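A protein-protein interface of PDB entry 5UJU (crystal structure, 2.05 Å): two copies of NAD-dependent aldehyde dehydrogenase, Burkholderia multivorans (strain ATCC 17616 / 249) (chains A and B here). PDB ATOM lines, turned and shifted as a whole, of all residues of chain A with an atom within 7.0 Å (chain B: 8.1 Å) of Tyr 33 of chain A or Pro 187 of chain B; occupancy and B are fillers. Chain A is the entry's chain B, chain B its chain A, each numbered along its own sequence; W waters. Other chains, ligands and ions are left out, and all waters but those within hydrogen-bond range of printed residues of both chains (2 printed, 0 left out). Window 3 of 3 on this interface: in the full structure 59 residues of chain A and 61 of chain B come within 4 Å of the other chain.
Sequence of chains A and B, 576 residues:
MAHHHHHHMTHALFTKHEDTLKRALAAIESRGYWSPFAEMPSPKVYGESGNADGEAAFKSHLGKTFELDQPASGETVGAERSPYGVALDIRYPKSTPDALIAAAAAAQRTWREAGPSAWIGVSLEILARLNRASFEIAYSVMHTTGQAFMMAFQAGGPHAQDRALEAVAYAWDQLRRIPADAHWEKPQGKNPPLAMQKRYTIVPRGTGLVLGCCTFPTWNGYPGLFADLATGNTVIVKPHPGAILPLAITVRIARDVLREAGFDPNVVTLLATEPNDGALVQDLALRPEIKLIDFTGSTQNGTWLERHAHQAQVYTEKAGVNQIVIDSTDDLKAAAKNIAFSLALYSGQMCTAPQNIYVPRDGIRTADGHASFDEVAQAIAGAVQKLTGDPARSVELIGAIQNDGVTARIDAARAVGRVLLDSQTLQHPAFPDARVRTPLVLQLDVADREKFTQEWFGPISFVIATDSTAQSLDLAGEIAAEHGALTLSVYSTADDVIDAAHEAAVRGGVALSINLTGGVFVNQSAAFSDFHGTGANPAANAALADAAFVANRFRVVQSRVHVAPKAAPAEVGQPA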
ATOM      1  N   ARG A  23     -18.912  10.149 -32.851  1.00  0.00           N
ATOM      2  CA  ARG A  23     -18.722   8.727 -32.599  1.00  0.00           C
ATOM      3  C   ARG A  23     -19.447   8.286 -31.330  1.00  0.00           C
ATOM      4  O   ARG A  23     -19.987   7.173 -31.272  1.00  0.00           O
ATOM      5  CB  ARG A  23     -17.224   8.429 -32.518  1.00  0.00           C
ATOM      6  CG  ARG A  23     -16.874   6.964 -32.395  1.00  0.00           C
ATOM      7  CD  ARG A  23     -17.255   6.184 -33.640  1.00  0.00           C
ATOM      8  NE  ARG A  23     -17.142   4.748 -33.415  1.00  0.00           N
ATOM      9  CZ  ARG A  23     -18.096   4.012 -32.849  1.00  0.00           C
ATOM     10  NH1 ARG A  23     -19.228   4.585 -32.452  1.00  0.00           N
ATOM     11  NH2 ARG A  23     -17.921   2.704 -32.684  1.00  0.00           N
ATOM     12  N   ALA A  27     -22.411   5.581 -30.725  1.00  0.00           N
ATOM     13  CA  ALA A  27     -22.182   4.506 -29.764  1.00  0.00           C
ATOM     14  C   ALA A  27     -23.382   4.308 -28.841  1.00  0.00           C
ATOM     15  O   ALA A  27     -23.760   3.165 -28.554  1.00  0.00           O
ATOM     16  CB  ALA A  27     -20.911   4.781 -28.956  1.00  0.00           C
ATOM     17  N   SER A  30     -26.063   2.440 -31.013  1.00  0.00           N
ATOM     18  CA  SER A  30     -25.824   1.066 -31.456  1.00  0.00           C
ATOM     19  C   SER A  30     -25.498   0.140 -30.279  1.00  0.00           C
ATOM     20  O   SER A  30     -25.919  -1.019 -30.271  1.00  0.00           O
ATOM     21  CB  SER A  30     -24.714   1.025 -32.515  1.00  0.00           C
ATOM     22  OG  SER A  30     -23.438   1.280 -31.962  1.00  0.00           O
ATOM     23  N   ARG A  31     -24.768   0.636 -29.277  1.00  0.00           N
ATOM     24  CA  ARG A  31     -24.520  -0.075 -28.020  1.00  0.00           C
ATOM     25  C   ARG A  31     -23.614  -1.291 -28.201  1.00  0.00           C
ATOM     26  O   ARG A  31     -23.669  -2.244 -27.415  1.00  0.00           O
ATOM     27  CB  ARG A  31     -25.834  -0.451 -27.320  1.00  0.00           C
ATOM     28  CG  ARG A  31     -26.677   0.799 -27.044  1.00  0.00           C
ATOM     29  CD  ARG A  31     -27.740   0.629 -25.969  1.00  0.00           C
ATOM     30  NE  ARG A  31     -27.213   0.638 -24.603  1.00  0.00           N
ATOM     31  CZ  ARG A  31     -26.845   1.727 -23.932  1.00  0.00           C
ATOM     32  NH1 ARG A  31     -26.912   2.944 -24.496  1.00  0.00           N
ATOM     33  NH2 ARG A  31     -26.398   1.599 -22.686  1.00  0.00           N
ATOM     34  N   GLY A  32     -22.763  -1.264 -29.222  1.00  0.00           N
ATOM     35  CA  GLY A  32     -21.635  -2.168 -29.284  1.00  0.00           C
ATOM     36  C   GLY A  32     -20.527  -1.710 -28.348  1.00  0.00           C
ATOM     37  O   GLY A  32     -20.721  -0.871 -27.467  1.00  0.00           O
ATOM     38  N   TYR A  33     -19.336  -2.280 -28.549  1.00  0.00           N
ATOM     39  CA  TYR A  33     -18.190  -1.885 -27.739  1.00  0.00           C
ATOM     40  C   TYR A  33     -17.538  -0.633 -28.317  1.00  0.00           C
ATOM     41  O   TYR A  33     -17.251  -0.575 -29.514  1.00  0.00           O
ATOM     42  CB  TYR A  33     -17.142  -3.000 -27.647  1.00  0.00           C
ATOM     43  CG  TYR A  33     -15.896  -2.459 -26.967  1.00  0.00           C
ATOM     44  CD1 TYR A  33     -15.926  -2.108 -25.622  1.00  0.00           C
ATOM     45  CD2 TYR A  33     -14.721  -2.238 -27.677  1.00  0.00           C
ATOM     46  CE1 TYR A  33     -14.817  -1.577 -24.991  1.00  0.00           C
ATOM     47  CE2 TYR A  33     -13.594  -1.697 -27.049  1.00  0.00           C
ATOM     48  CZ  TYR A  33     -13.657  -1.373 -25.705  1.00  0.00           C
ATOM     49  OH  TYR A  33     -12.563  -0.854 -25.060  1.00  0.00           O
ATOM     50  N   TRP A  34     -17.299   0.363 -27.465  1.00  0.00           N
ATOM     51  CA  TRP A  34     -16.553   1.548 -27.870  1.00  0.00           C
ATOM     52  C   TRP A  34     -16.096   2.298 -26.628  1.00  0.00           C
ATOM     53  O   TRP A  34     -16.830   2.387 -25.640  1.00  0.00           O
ATOM     54  CB  TRP A  34     -17.369   2.485 -28.770  1.00  0.00           C
ATOM     55  CG  TRP A  34     -16.577   3.702 -29.196  1.00  0.00           C
ATOM     56  CD1 TRP A  34     -15.550   3.727 -30.092  1.00  0.00           C
ATOM     57  CD2 TRP A  34     -16.746   5.056 -28.744  1.00  0.00           C
ATOM     58  NE1 TRP A  34     -15.064   5.008 -30.227  1.00  0.00           N
ATOM     59  CE2 TRP A  34     -15.782   5.845 -29.413  1.00  0.00           C
ATOM     60  CE3 TRP A  34     -17.616   5.680 -27.841  1.00  0.00           C
ATOM     61  CZ2 TRP A  34     -15.664   7.226 -29.211  1.00  0.00           C
ATOM     62  CZ3 TRP A  34     -17.504   7.053 -27.641  1.00  0.00           C
ATOM     63  CH2 TRP A  34     -16.531   7.813 -28.329  1.00  0.00           C
ATOM     64  N   SER A  35     -14.889   2.848 -26.703  1.00  0.00           N
ATOM     65  CA  SER A  35     -14.280   3.648 -25.653  1.00  0.00           C
ATOM     66  C   SER A  35     -13.200   4.524 -26.264  1.00  0.00           C
ATOM     67  O   SER A  35     -12.281   4.013 -26.914  1.00  0.00           O
ATOM     68  CB  SER A  35     -13.672   2.762 -24.567  1.00  0.00           C
ATOM     69  OG  SER A  35     -12.912   3.552 -23.667  1.00  0.00           O
ATOM     70  N   PRO A  36     -13.274   5.846 -26.090  1.00  0.00           N
ATOM     71  CA  PRO A  36     -12.206   6.715 -26.606  1.00  0.00           C
ATOM     72  C   PRO A  36     -11.006   6.828 -25.683  1.00  0.00           C
ATOM     73  O   PRO A  36      -9.989   7.403 -26.088  1.00  0.00           O
ATOM     74  CB  PRO A  36     -12.911   8.067 -26.754  1.00  0.00           C
ATOM     75  CG  PRO A  36     -13.894   8.072 -25.642  1.00  0.00           C
ATOM     76  CD  PRO A  36     -14.371   6.622 -25.490  1.00  0.00           C
ATOM     77  N   PHE A  37     -11.082   6.288 -24.473  1.00  0.00           N
ATOM     78  CA  PHE A  37     -10.034   6.430 -23.472  1.00  0.00           C
ATOM     79  C   PHE A  37      -9.411   5.071 -23.188  1.00  0.00           C
ATOM     80  O   PHE A  37     -10.106   4.148 -22.752  1.00  0.00           O
ATOM     81  CB  PHE A  37     -10.599   7.054 -22.197  1.00  0.00           C
ATOM     82  CG  PHE A  37     -11.222   8.405 -22.416  1.00  0.00           C
ATOM     83  CD1 PHE A  37     -10.451   9.469 -22.843  1.00  0.00           C
ATOM     84  CD2 PHE A  37     -12.579   8.609 -22.201  1.00  0.00           C
ATOM     85  CE1 PHE A  37     -11.014  10.722 -23.042  1.00  0.00           C
ATOM     86  CE2 PHE A  37     -13.151   9.860 -22.396  1.00  0.00           C
ATOM     87  CZ  PHE A  37     -12.370  10.915 -22.815  1.00  0.00           C
ATOM     88  N   GLU A  39      -8.040   2.151 -21.511  1.00  0.00           N
ATOM     89  CA  GLU A  39      -8.167   1.718 -20.128  1.00  0.00           C
ATOM     90  C   GLU A  39      -6.882   1.110 -19.584  1.00  0.00           C
ATOM     91  O   GLU A  39      -6.735   1.010 -18.359  1.00  0.00           O
ATOM     92  CB  GLU A  39      -9.315   0.709 -19.998  1.00  0.00           C
ATOM     93  CG  GLU A  39      -9.072  -0.598 -20.750  1.00  0.00           C
ATOM     94  CD  GLU A  39     -10.131  -1.656 -20.449  1.00  0.00           C
ATOM     95  OE1 GLU A  39     -11.138  -1.349 -19.768  1.00  0.00           O
ATOM     96  OE2 GLU A  39      -9.965  -2.794 -20.920  1.00  0.00           O
ATOM     97  N   ASP A 162     -15.039   7.626 -19.652  1.00  0.00           N
ATOM     98  CA  ASP A 162     -16.053   7.055 -20.542  1.00  0.00           C
ATOM     99  C   ASP A 162     -17.462   7.440 -20.096  1.00  0.00           C
ATOM    100  O   ASP A 162     -18.261   7.958 -20.886  1.00  0.00           O
ATOM    101  CB  ASP A 162     -15.937   5.524 -20.600  1.00  0.00           C
ATOM    102  CG  ASP A 162     -14.733   5.038 -21.391  1.00  0.00           C
ATOM    103  OD1 ASP A 162     -14.156   5.806 -22.190  1.00  0.00           O
ATOM    104  OD2 ASP A 162     -14.381   3.849 -21.228  1.00  0.00           O
ATOM    105  N   ALA A 526     -19.817  -1.684 -19.116  1.00  0.00           N
ATOM    106  CA  ALA A 526     -19.160  -0.877 -20.135  1.00  0.00           C
ATOM    107  C   ALA A 526     -20.039   0.315 -20.496  1.00  0.00           C
ATOM    108  O   ALA A 526     -21.215   0.147 -20.838  1.00  0.00           O
ATOM    109  CB  ALA A 526     -18.866  -1.721 -21.376  1.00  0.00           C
ATOM    110  N   ALA A 527     -19.466   1.517 -20.432  1.00  0.00           N
ATOM    111  CA  ALA A 527     -20.155   2.685 -20.958  1.00  0.00           C
ATOM    112  C   ALA A 527     -20.511   2.454 -22.424  1.00  0.00           C
ATOM    113  O   ALA A 527     -19.847   1.690 -23.132  1.00  0.00           O
ATOM    114  CB  ALA A 527     -19.280   3.927 -20.813  1.00  0.00           C
ATOM    115  N   PHE A 528     -21.576   3.118 -22.875  1.00  0.00           N
ATOM    116  CA  PHE A 528     -22.064   3.056 -24.251  1.00  0.00           C
ATOM    117  C   PHE A 528     -22.665   1.702 -24.612  1.00  0.00           C
ATOM    118  O   PHE A 528     -22.919   1.448 -25.795  1.00  0.00           O
ATOM    119  CB  PHE A 528     -20.958   3.423 -25.261  1.00  0.00           C
ATOM    120  CG  PHE A 528     -20.281   4.734 -24.950  1.00  0.00           C
ATOM    121  CD1 PHE A 528     -20.912   5.937 -25.245  1.00  0.00           C
ATOM    122  CD2 PHE A 528     -19.039   4.766 -24.333  1.00  0.00           C
ATOM    123  CE1 PHE A 528     -20.305   7.155 -24.943  1.00  0.00           C
ATOM    124  CE2 PHE A 528     -18.426   5.976 -24.029  1.00  0.00           C
ATOM    125  CZ  PHE A 528     -19.065   7.165 -24.333  1.00  0.00           C
ATOM    126  N   SER A 529     -22.909   0.829 -23.633  1.00  0.00           N
ATOM    127  CA  SER A 529     -23.599  -0.426 -23.903  1.00  0.00           C
ATOM    128  C   SER A 529     -24.444  -0.832 -22.701  1.00  0.00           C
ATOM    129  O   SER A 529     -25.627  -1.156 -22.851  1.00  0.00           O
ATOM    130  CB  SER A 529     -22.605  -1.532 -24.272  1.00  0.00           C
ATOM    131  OG  SER A 529     -23.278  -2.742 -24.605  1.00  0.00           O
ATOM    132  N   ALA B 182     -27.748  -5.872 -29.243  1.00  0.00           N
ATOM    133  CA  ALA B 182     -26.476  -5.371 -29.735  1.00  0.00           C
ATOM    134  C   ALA B 182     -25.439  -6.475 -29.605  1.00  0.00           C
ATOM    135  O   ALA B 182     -25.468  -7.255 -28.646  1.00  0.00           O
ATOM    136  CB  ALA B 182     -26.027  -4.115 -28.964  1.00  0.00           C
ATOM    137  N   HIS B 183     -24.530  -6.541 -30.575  1.00  0.00           N
ATOM    138  CA  HIS B 183     -23.366  -7.412 -30.486  1.00  0.00           C
ATOM    139  C   HIS B 183     -22.211  -6.599 -29.913  1.00  0.00           C
ATOM    140  O   HIS B 183     -21.698  -5.684 -30.567  1.00  0.00           O
ATOM    141  CB  HIS B 183     -22.994  -7.995 -31.843  1.00  0.00           C
ATOM    142  CG  HIS B 183     -21.831  -8.933 -31.786  1.00  0.00           C
ATOM    143  ND1 HIS B 183     -21.963 -10.265 -31.462  1.00  0.00           N
ATOM    144  CD2 HIS B 183     -20.508  -8.726 -31.993  1.00  0.00           C
ATOM    145  CE1 HIS B 183     -20.776 -10.844 -31.487  1.00  0.00           C
ATOM    146  NE2 HIS B 183     -19.875  -9.933 -31.807  1.00  0.00           N
ATOM    147  N   TRP B 184     -21.790  -6.953 -28.707  1.00  0.00           N
ATOM    148  CA  TRP B 184     -20.755  -6.239 -27.974  1.00  0.00           C
ATOM    149  C   TRP B 184     -19.494  -7.087 -28.033  1.00  0.00           C
ATOM    150  O   TRP B 184     -19.444  -8.171 -27.437  1.00  0.00           O
ATOM    151  CB  TRP B 184     -21.202  -6.007 -26.535  1.00  0.00           C
ATOM    152  CG  TRP B 184     -20.293  -5.156 -25.719  1.00  0.00           C
ATOM    153  CD1 TRP B 184     -20.376  -3.800 -25.559  1.00  0.00           C
ATOM    154  CD2 TRP B 184     -19.191  -5.588 -24.916  1.00  0.00           C
ATOM    155  NE1 TRP B 184     -19.382  -3.359 -24.718  1.00  0.00           N
ATOM    156  CE2 TRP B 184     -18.641  -4.433 -24.306  1.00  0.00           C
ATOM    157  CE3 TRP B 184     -18.608  -6.832 -24.654  1.00  0.00           C
ATOM    158  CZ2 TRP B 184     -17.529  -4.489 -23.458  1.00  0.00           C
ATOM    159  CZ3 TRP B 184     -17.504  -6.885 -23.806  1.00  0.00           C
ATOM    160  CH2 TRP B 184     -16.978  -5.719 -23.218  1.00  0.00           C
ATOM    161  N   GLU B 185     -18.481  -6.605 -28.749  1.00  0.00           N
ATOM    162  CA  GLU B 185     -17.250  -7.366 -28.934  1.00  0.00           C
ATOM    163  C   GLU B 185     -16.056  -6.478 -28.629  1.00  0.00           C
ATOM    164  O   GLU B 185     -15.845  -5.463 -29.301  1.00  0.00           O
ATOM    165  CB  GLU B 185     -17.142  -7.941 -30.347  1.00  0.00           C
ATOM    166  CG  GLU B 185     -15.878  -8.777 -30.532  1.00  0.00           C
ATOM    167  CD  GLU B 185     -15.901  -9.641 -31.786  1.00  0.00           C
ATOM    168  OE1 GLU B 185     -16.996 -10.073 -32.208  1.00  0.00           O
ATOM    169  OE2 GLU B 185     -14.813  -9.885 -32.344  1.00  0.00           O
ATOM    170  N   LYS B 186     -15.256  -6.892 -27.650  1.00  0.00           N
ATOM    171  CA  LYS B 186     -14.160  -6.083 -27.135  1.00  0.00           C
ATOM    172  C   LYS B 186     -12.840  -6.779 -27.407  1.00  0.00           C
ATOM    173  O   LYS B 186     -12.594  -7.866 -26.855  1.00  0.00           O
ATOM    174  CB  LYS B 186     -14.320  -5.827 -25.635  1.00  0.00           C
ATOM    175  CG  LYS B 186     -13.134  -5.094 -25.020  1.00  0.00           C
ATOM    176  CD  LYS B 186     -13.431  -4.683 -23.594  1.00  0.00           C
ATOM    177  CE  LYS B 186     -12.208  -4.098 -22.915  1.00  0.00           C
ATOM    178  NZ  LYS B 186     -12.516  -3.719 -21.502  1.00  0.00           N
ATOM    179  N   PRO B 187     -11.967  -6.202 -28.233  1.00  0.00           N
ATOM    180  CA  PRO B 187     -10.688  -6.853 -28.521  1.00  0.00           C
ATOM    181  C   PRO B 187      -9.855  -7.029 -27.261  1.00  0.00           C
ATOM    182  O   PRO B 187      -9.925  -6.233 -26.322  1.00  0.00           O
ATOM    183  CB  PRO B 187     -10.014  -5.890 -29.507  1.00  0.00           C
ATOM    184  CG  PRO B 187     -11.154  -5.117 -30.123  1.00  0.00           C
ATOM    185  CD  PRO B 187     -12.158  -4.965 -29.016  1.00  0.00           C
ATOM    186  N   GLN B 188      -9.049  -8.082 -27.259  1.00  0.00           N
ATOM    187  CA  GLN B 188      -8.179  -8.410 -26.137  1.00  0.00           C
ATOM    188  C   GLN B 188      -6.780  -8.613 -26.696  1.00  0.00           C
ATOM    189  O   GLN B 188      -6.578  -9.478 -27.553  1.00  0.00           O
ATOM    190  CB  GLN B 188      -8.665  -9.668 -25.409  1.00  0.00           C
ATOM    191  CG  GLN B 188     -10.051  -9.560 -24.813  1.00  0.00           C
ATOM    192  CD  GLN B 188     -10.095  -8.710 -23.559  1.00  0.00           C
ATOM    193  OE1 GLN B 188     -10.125  -7.479 -23.630  1.00  0.00           O
ATOM    194  NE2 GLN B 188     -10.107  -9.360 -22.401  1.00  0.00           N
ATOM    195  N   GLY B 189      -5.827  -7.812 -26.224  1.00  0.00           N
ATOM    196  CA  GLY B 189      -4.439  -7.898 -26.647  1.00  0.00           C
ATOM    197  C   GLY B 189      -3.873  -9.297 -26.794  1.00  0.00           C
ATOM    198  O   GLY B 189      -3.386  -9.878 -25.819  1.00  0.00           O
ATOM    199  N   LYS B 190      -3.938  -9.845 -28.013  1.00  0.00           N
ATOM    200  CA  LYS B 190      -3.400 -11.171 -28.335  1.00  0.00           C
ATOM    201  C   LYS B 190      -4.101 -12.282 -27.551  1.00  0.00           C
ATOM    202  O   LYS B 190      -3.494 -13.300 -27.214  1.00  0.00           O
ATOM    203  CB  LYS B 190      -1.884 -11.232 -28.114  1.00  0.00           C
ATOM    204  N   ASN B 191      -5.380 -12.098 -27.256  1.00  0.00           N
ATOM    205  CA  ASN B 191      -6.218 -13.102 -26.614  1.00  0.00           C
ATOM    206  C   ASN B 191      -7.560 -13.092 -27.338  1.00  0.00           C
ATOM    207  O   ASN B 191      -7.802 -12.186 -28.146  1.00  0.00           O
ATOM    208  CB  ASN B 191      -6.363 -12.808 -25.119  1.00  0.00           C
ATOM    209  N   PRO B 192      -8.442 -14.066 -27.122  1.00  0.00           N
ATOM    210  CA  PRO B 192      -9.737 -14.037 -27.819  1.00  0.00           C
ATOM    211  C   PRO B 192     -10.560 -12.848 -27.364  1.00  0.00           C
ATOM    212  O   PRO B 192     -10.553 -12.498 -26.174  1.00  0.00           O
ATOM    213  CB  PRO B 192     -10.403 -15.362 -27.411  1.00  0.00           C
ATOM    214  CG  PRO B 192      -9.302 -16.213 -26.911  1.00  0.00           C
ATOM    215  CD  PRO B 192      -8.294 -15.288 -26.309  1.00  0.00           C
ATOM    216  N   PRO B 193     -11.285 -12.201 -28.273  1.00  0.00           N
ATOM    217  CA  PRO B 193     -12.090 -11.044 -27.870  1.00  0.00           C
ATOM    218  C   PRO B 193     -13.199 -11.455 -26.914  1.00  0.00           C
ATOM    219  O   PRO B 193     -13.730 -12.566 -26.976  1.00  0.00           O
ATOM    220  CB  PRO B 193     -12.659 -10.523 -29.198  1.00  0.00           C
ATOM    221  CG  PRO B 193     -12.571 -11.688 -30.137  1.00  0.00           C
ATOM    222  CD  PRO B 193     -11.343 -12.440 -29.725  1.00  0.00           C
ATOM    223  N   LEU B 194     -13.542 -10.545 -26.008  1.00  0.00           N
ATOM    224  CA  LEU B 194     -14.780 -10.699 -25.264  1.00  0.00           C
ATOM    225  C   LEU B 194     -15.937 -10.388 -26.199  1.00  0.00           C
ATOM    226  O   LEU B 194     -15.998  -9.300 -26.779  1.00  0.00           O
ATOM    227  CB  LEU B 194     -14.812  -9.779 -24.050  1.00  0.00           C
ATOM    228  CG  LEU B 194     -13.641  -9.805 -23.075  1.00  0.00           C
ATOM    229  CD1 LEU B 194     -13.919  -8.805 -21.971  1.00  0.00           C
ATOM    230  CD2 LEU B 194     -13.427 -11.191 -22.503  1.00  0.00           C
ATOM    231  N   ALA B 195     -16.857 -11.334 -26.348  1.00  0.00           N
ATOM    232  CA  ALA B 195     -18.006 -11.151 -27.221  1.00  0.00           C
ATOM    233  C   ALA B 195     -19.258 -11.509 -26.443  1.00  0.00           C
ATOM    234  O   ALA B 195     -19.362 -12.613 -25.894  1.00  0.00           O
ATOM    235  CB  ALA B 195     -17.881 -12.003 -28.486  1.00  0.00           C
ATOM    236  N   MET B 196     -20.199 -10.574 -26.389  1.00  0.00           N
ATOM    237  CA  MET B 196     -21.455 -10.791 -25.690  1.00  0.00           C
ATOM    238  C   MET B 196     -22.594 -10.282 -26.552  1.00  0.00           C
ATOM    239  O   MET B 196     -22.433  -9.346 -27.340  1.00  0.00           O
ATOM    240  CB  MET B 196     -21.484 -10.078 -24.337  1.00  0.00           C
ATOM    241  CG  MET B 196     -20.267 -10.331 -23.479  1.00  0.00           C
ATOM    242  SD  MET B 196     -20.548  -9.752 -21.799  1.00  0.00           S
ATOM    243  CE  MET B 196     -21.589 -11.079 -21.190  1.00  0.00           C
ATOM    244  N   LYS B 198     -26.065  -8.360 -26.122  1.00  0.00           N
ATOM    245  CA  LYS B 198     -26.886  -7.576 -25.225  1.00  0.00           C
ATOM    246  C   LYS B 198     -28.315  -7.605 -25.740  1.00  0.00           C
ATOM    247  O   LYS B 198     -28.550  -7.595 -26.949  1.00  0.00           O
ATOM    248  CB  LYS B 198     -26.387  -6.125 -25.135  1.00  0.00           C
ATOM    249  CG  LYS B 198     -24.882  -5.959 -24.927  1.00  0.00           C
ATOM    250  CD  LYS B 198     -24.440  -6.560 -23.597  1.00  0.00           C
ATOM    251  CE  LYS B 198     -22.944  -6.353 -23.336  1.00  0.00           C
ATOM    252  NZ  LYS B 198     -22.611  -4.947 -22.979  1.00  0.00           N
HETATM  253  O   HOH W   1     -19.360  -0.424 -25.044  1.00  0.00           O
HETATM  254  O   HOH W   2     -19.131  -4.239 -30.628  1.00  0.00           O
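The side-chain amino group (NZ) of Lys 186 of chain B lies within salt-bridge range of the side-chain carboxylate (OE2) of Glu 39 of chain A (2.8 Å). The side-chain amino group (NZ) of Lys 198 of chain B sits at hydrogen-bond distance from the side-chain hydroxyl (OG) of Ser 529 of chain A, 2.8 Å away.
Of the printed residues of chain B, Tyr 33 of chain A touches Trp 184, Glu 185, Lys 186 and Pro 187. Of chain A, only Tyr 33 (3.97 Å) comes within 4 Å of Pro 187 of chain B. Gly 32 of chain A touches just these residues of chain B: His 183 and Trp 184. Of the printed residues of chain B, Ala 526 of chain A touches Trp 184. Of the printed residues of chain B, Ser 30 of chain A touches Ala 182 (3.4 Å). Printed residues of chain A within 4 Å of Lys 198 of chain B: Ser 529. Printed residues of chain A within 4 Å of Lys 186 of chain B: Tyr 33 (3.7 Å) and Glu 39 (2.8 Å). Of the printed residues of chain A, His 183 of chain B touches Gly 32. Phe 528 of chain A touches none of the printed residues of chain B. Gly 189 of chain B touches none of the printed residues of chain A. The nearest residue of chain A that does not touch Pro 187 of chain B is Glu 39 of chain A (6.4 Å). The nearest printed residue of chain A that does not touch Lys 186 of chain B is Ala 526 of chain A (6.6 Å).
No position is printed for both chains. Of the 12 pairs that touch across the chains among the printed residues, none has its exchanged pair printed and touching as well.
The backbone carbonyl oxygen of Ala 182 of chain B is in hydrogen-bond range of the backbone NH of Lys 198 of chain B (2.8 Å). A ring nitrogen (NE2) of His 183 of chain B is in hydrogen-bond range of the side-chain carboxylate of Glu 185 of chain B, at 2.9 Å. N of Met 196 of chain B sits at hydrogen-bond distance from O of Trp 184 of chain B, at 2.7 Å. N of Lys 186 of chain B is in hydrogen-bond range of O of Leu 194 of chain B (2.7 Å). NH2 of Arg 31 of chain A sits at hydrogen-bond distance from O of Ser 529 of chain A.
Water W1 lies within hydrogen-bond range of O of Gly 32 of chain A, O of Ala 527 of chain A, NE1 of Trp 184 of chain B and N of Trp 34 of chain A. Water W2 lies within hydrogen-bond range of N of Tyr 33 of chain A (2.9 Å), O of His 183 of chain B (2.9 Å) and N of Glu 185 of chain B (3.1 Å).
Hydrophobic or aromatic side chains of chain A that line the printed part of chain B: Tyr 33 and Ala 526. Of the 16 printed residues of chain B, 7 touch a printed residue of chain A. Hydrophobic or aromatic side chains of chain B within 4 Å of the printed part of chain A: Ala 182, Trp 184 and Pro 187. Among the printed residues, 12 pairs touch across the chains.
Among the printed residues, pairs that only touch across the chains: Ser 30 of chain A with Ala 182 of chain B (3.4 Å), Arg 31 of chain A with Ala 182 of chain B (3.4 Å), Gly 32 of chain A with His 183 of chain B (3.7 Å), Gly 32 of chain A with Trp 184 of chain B (3.5 Å), Tyr 33 of chain A with Trp 184 of chain B (3.5 Å), Tyr 33 of chain A with Glu 185 of chain B (3.2 Å), Tyr 33 of chain A with Lys 186 of chain B (3.7 Å), Tyr 33 of chain A with Pro 187 of chain B (3.97 Å), Ala 526 of chain A with Trp 184 of chain B (3.7 Å) and Ser 529 of chain A with Trp 184 of chain B (3.2 Å).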
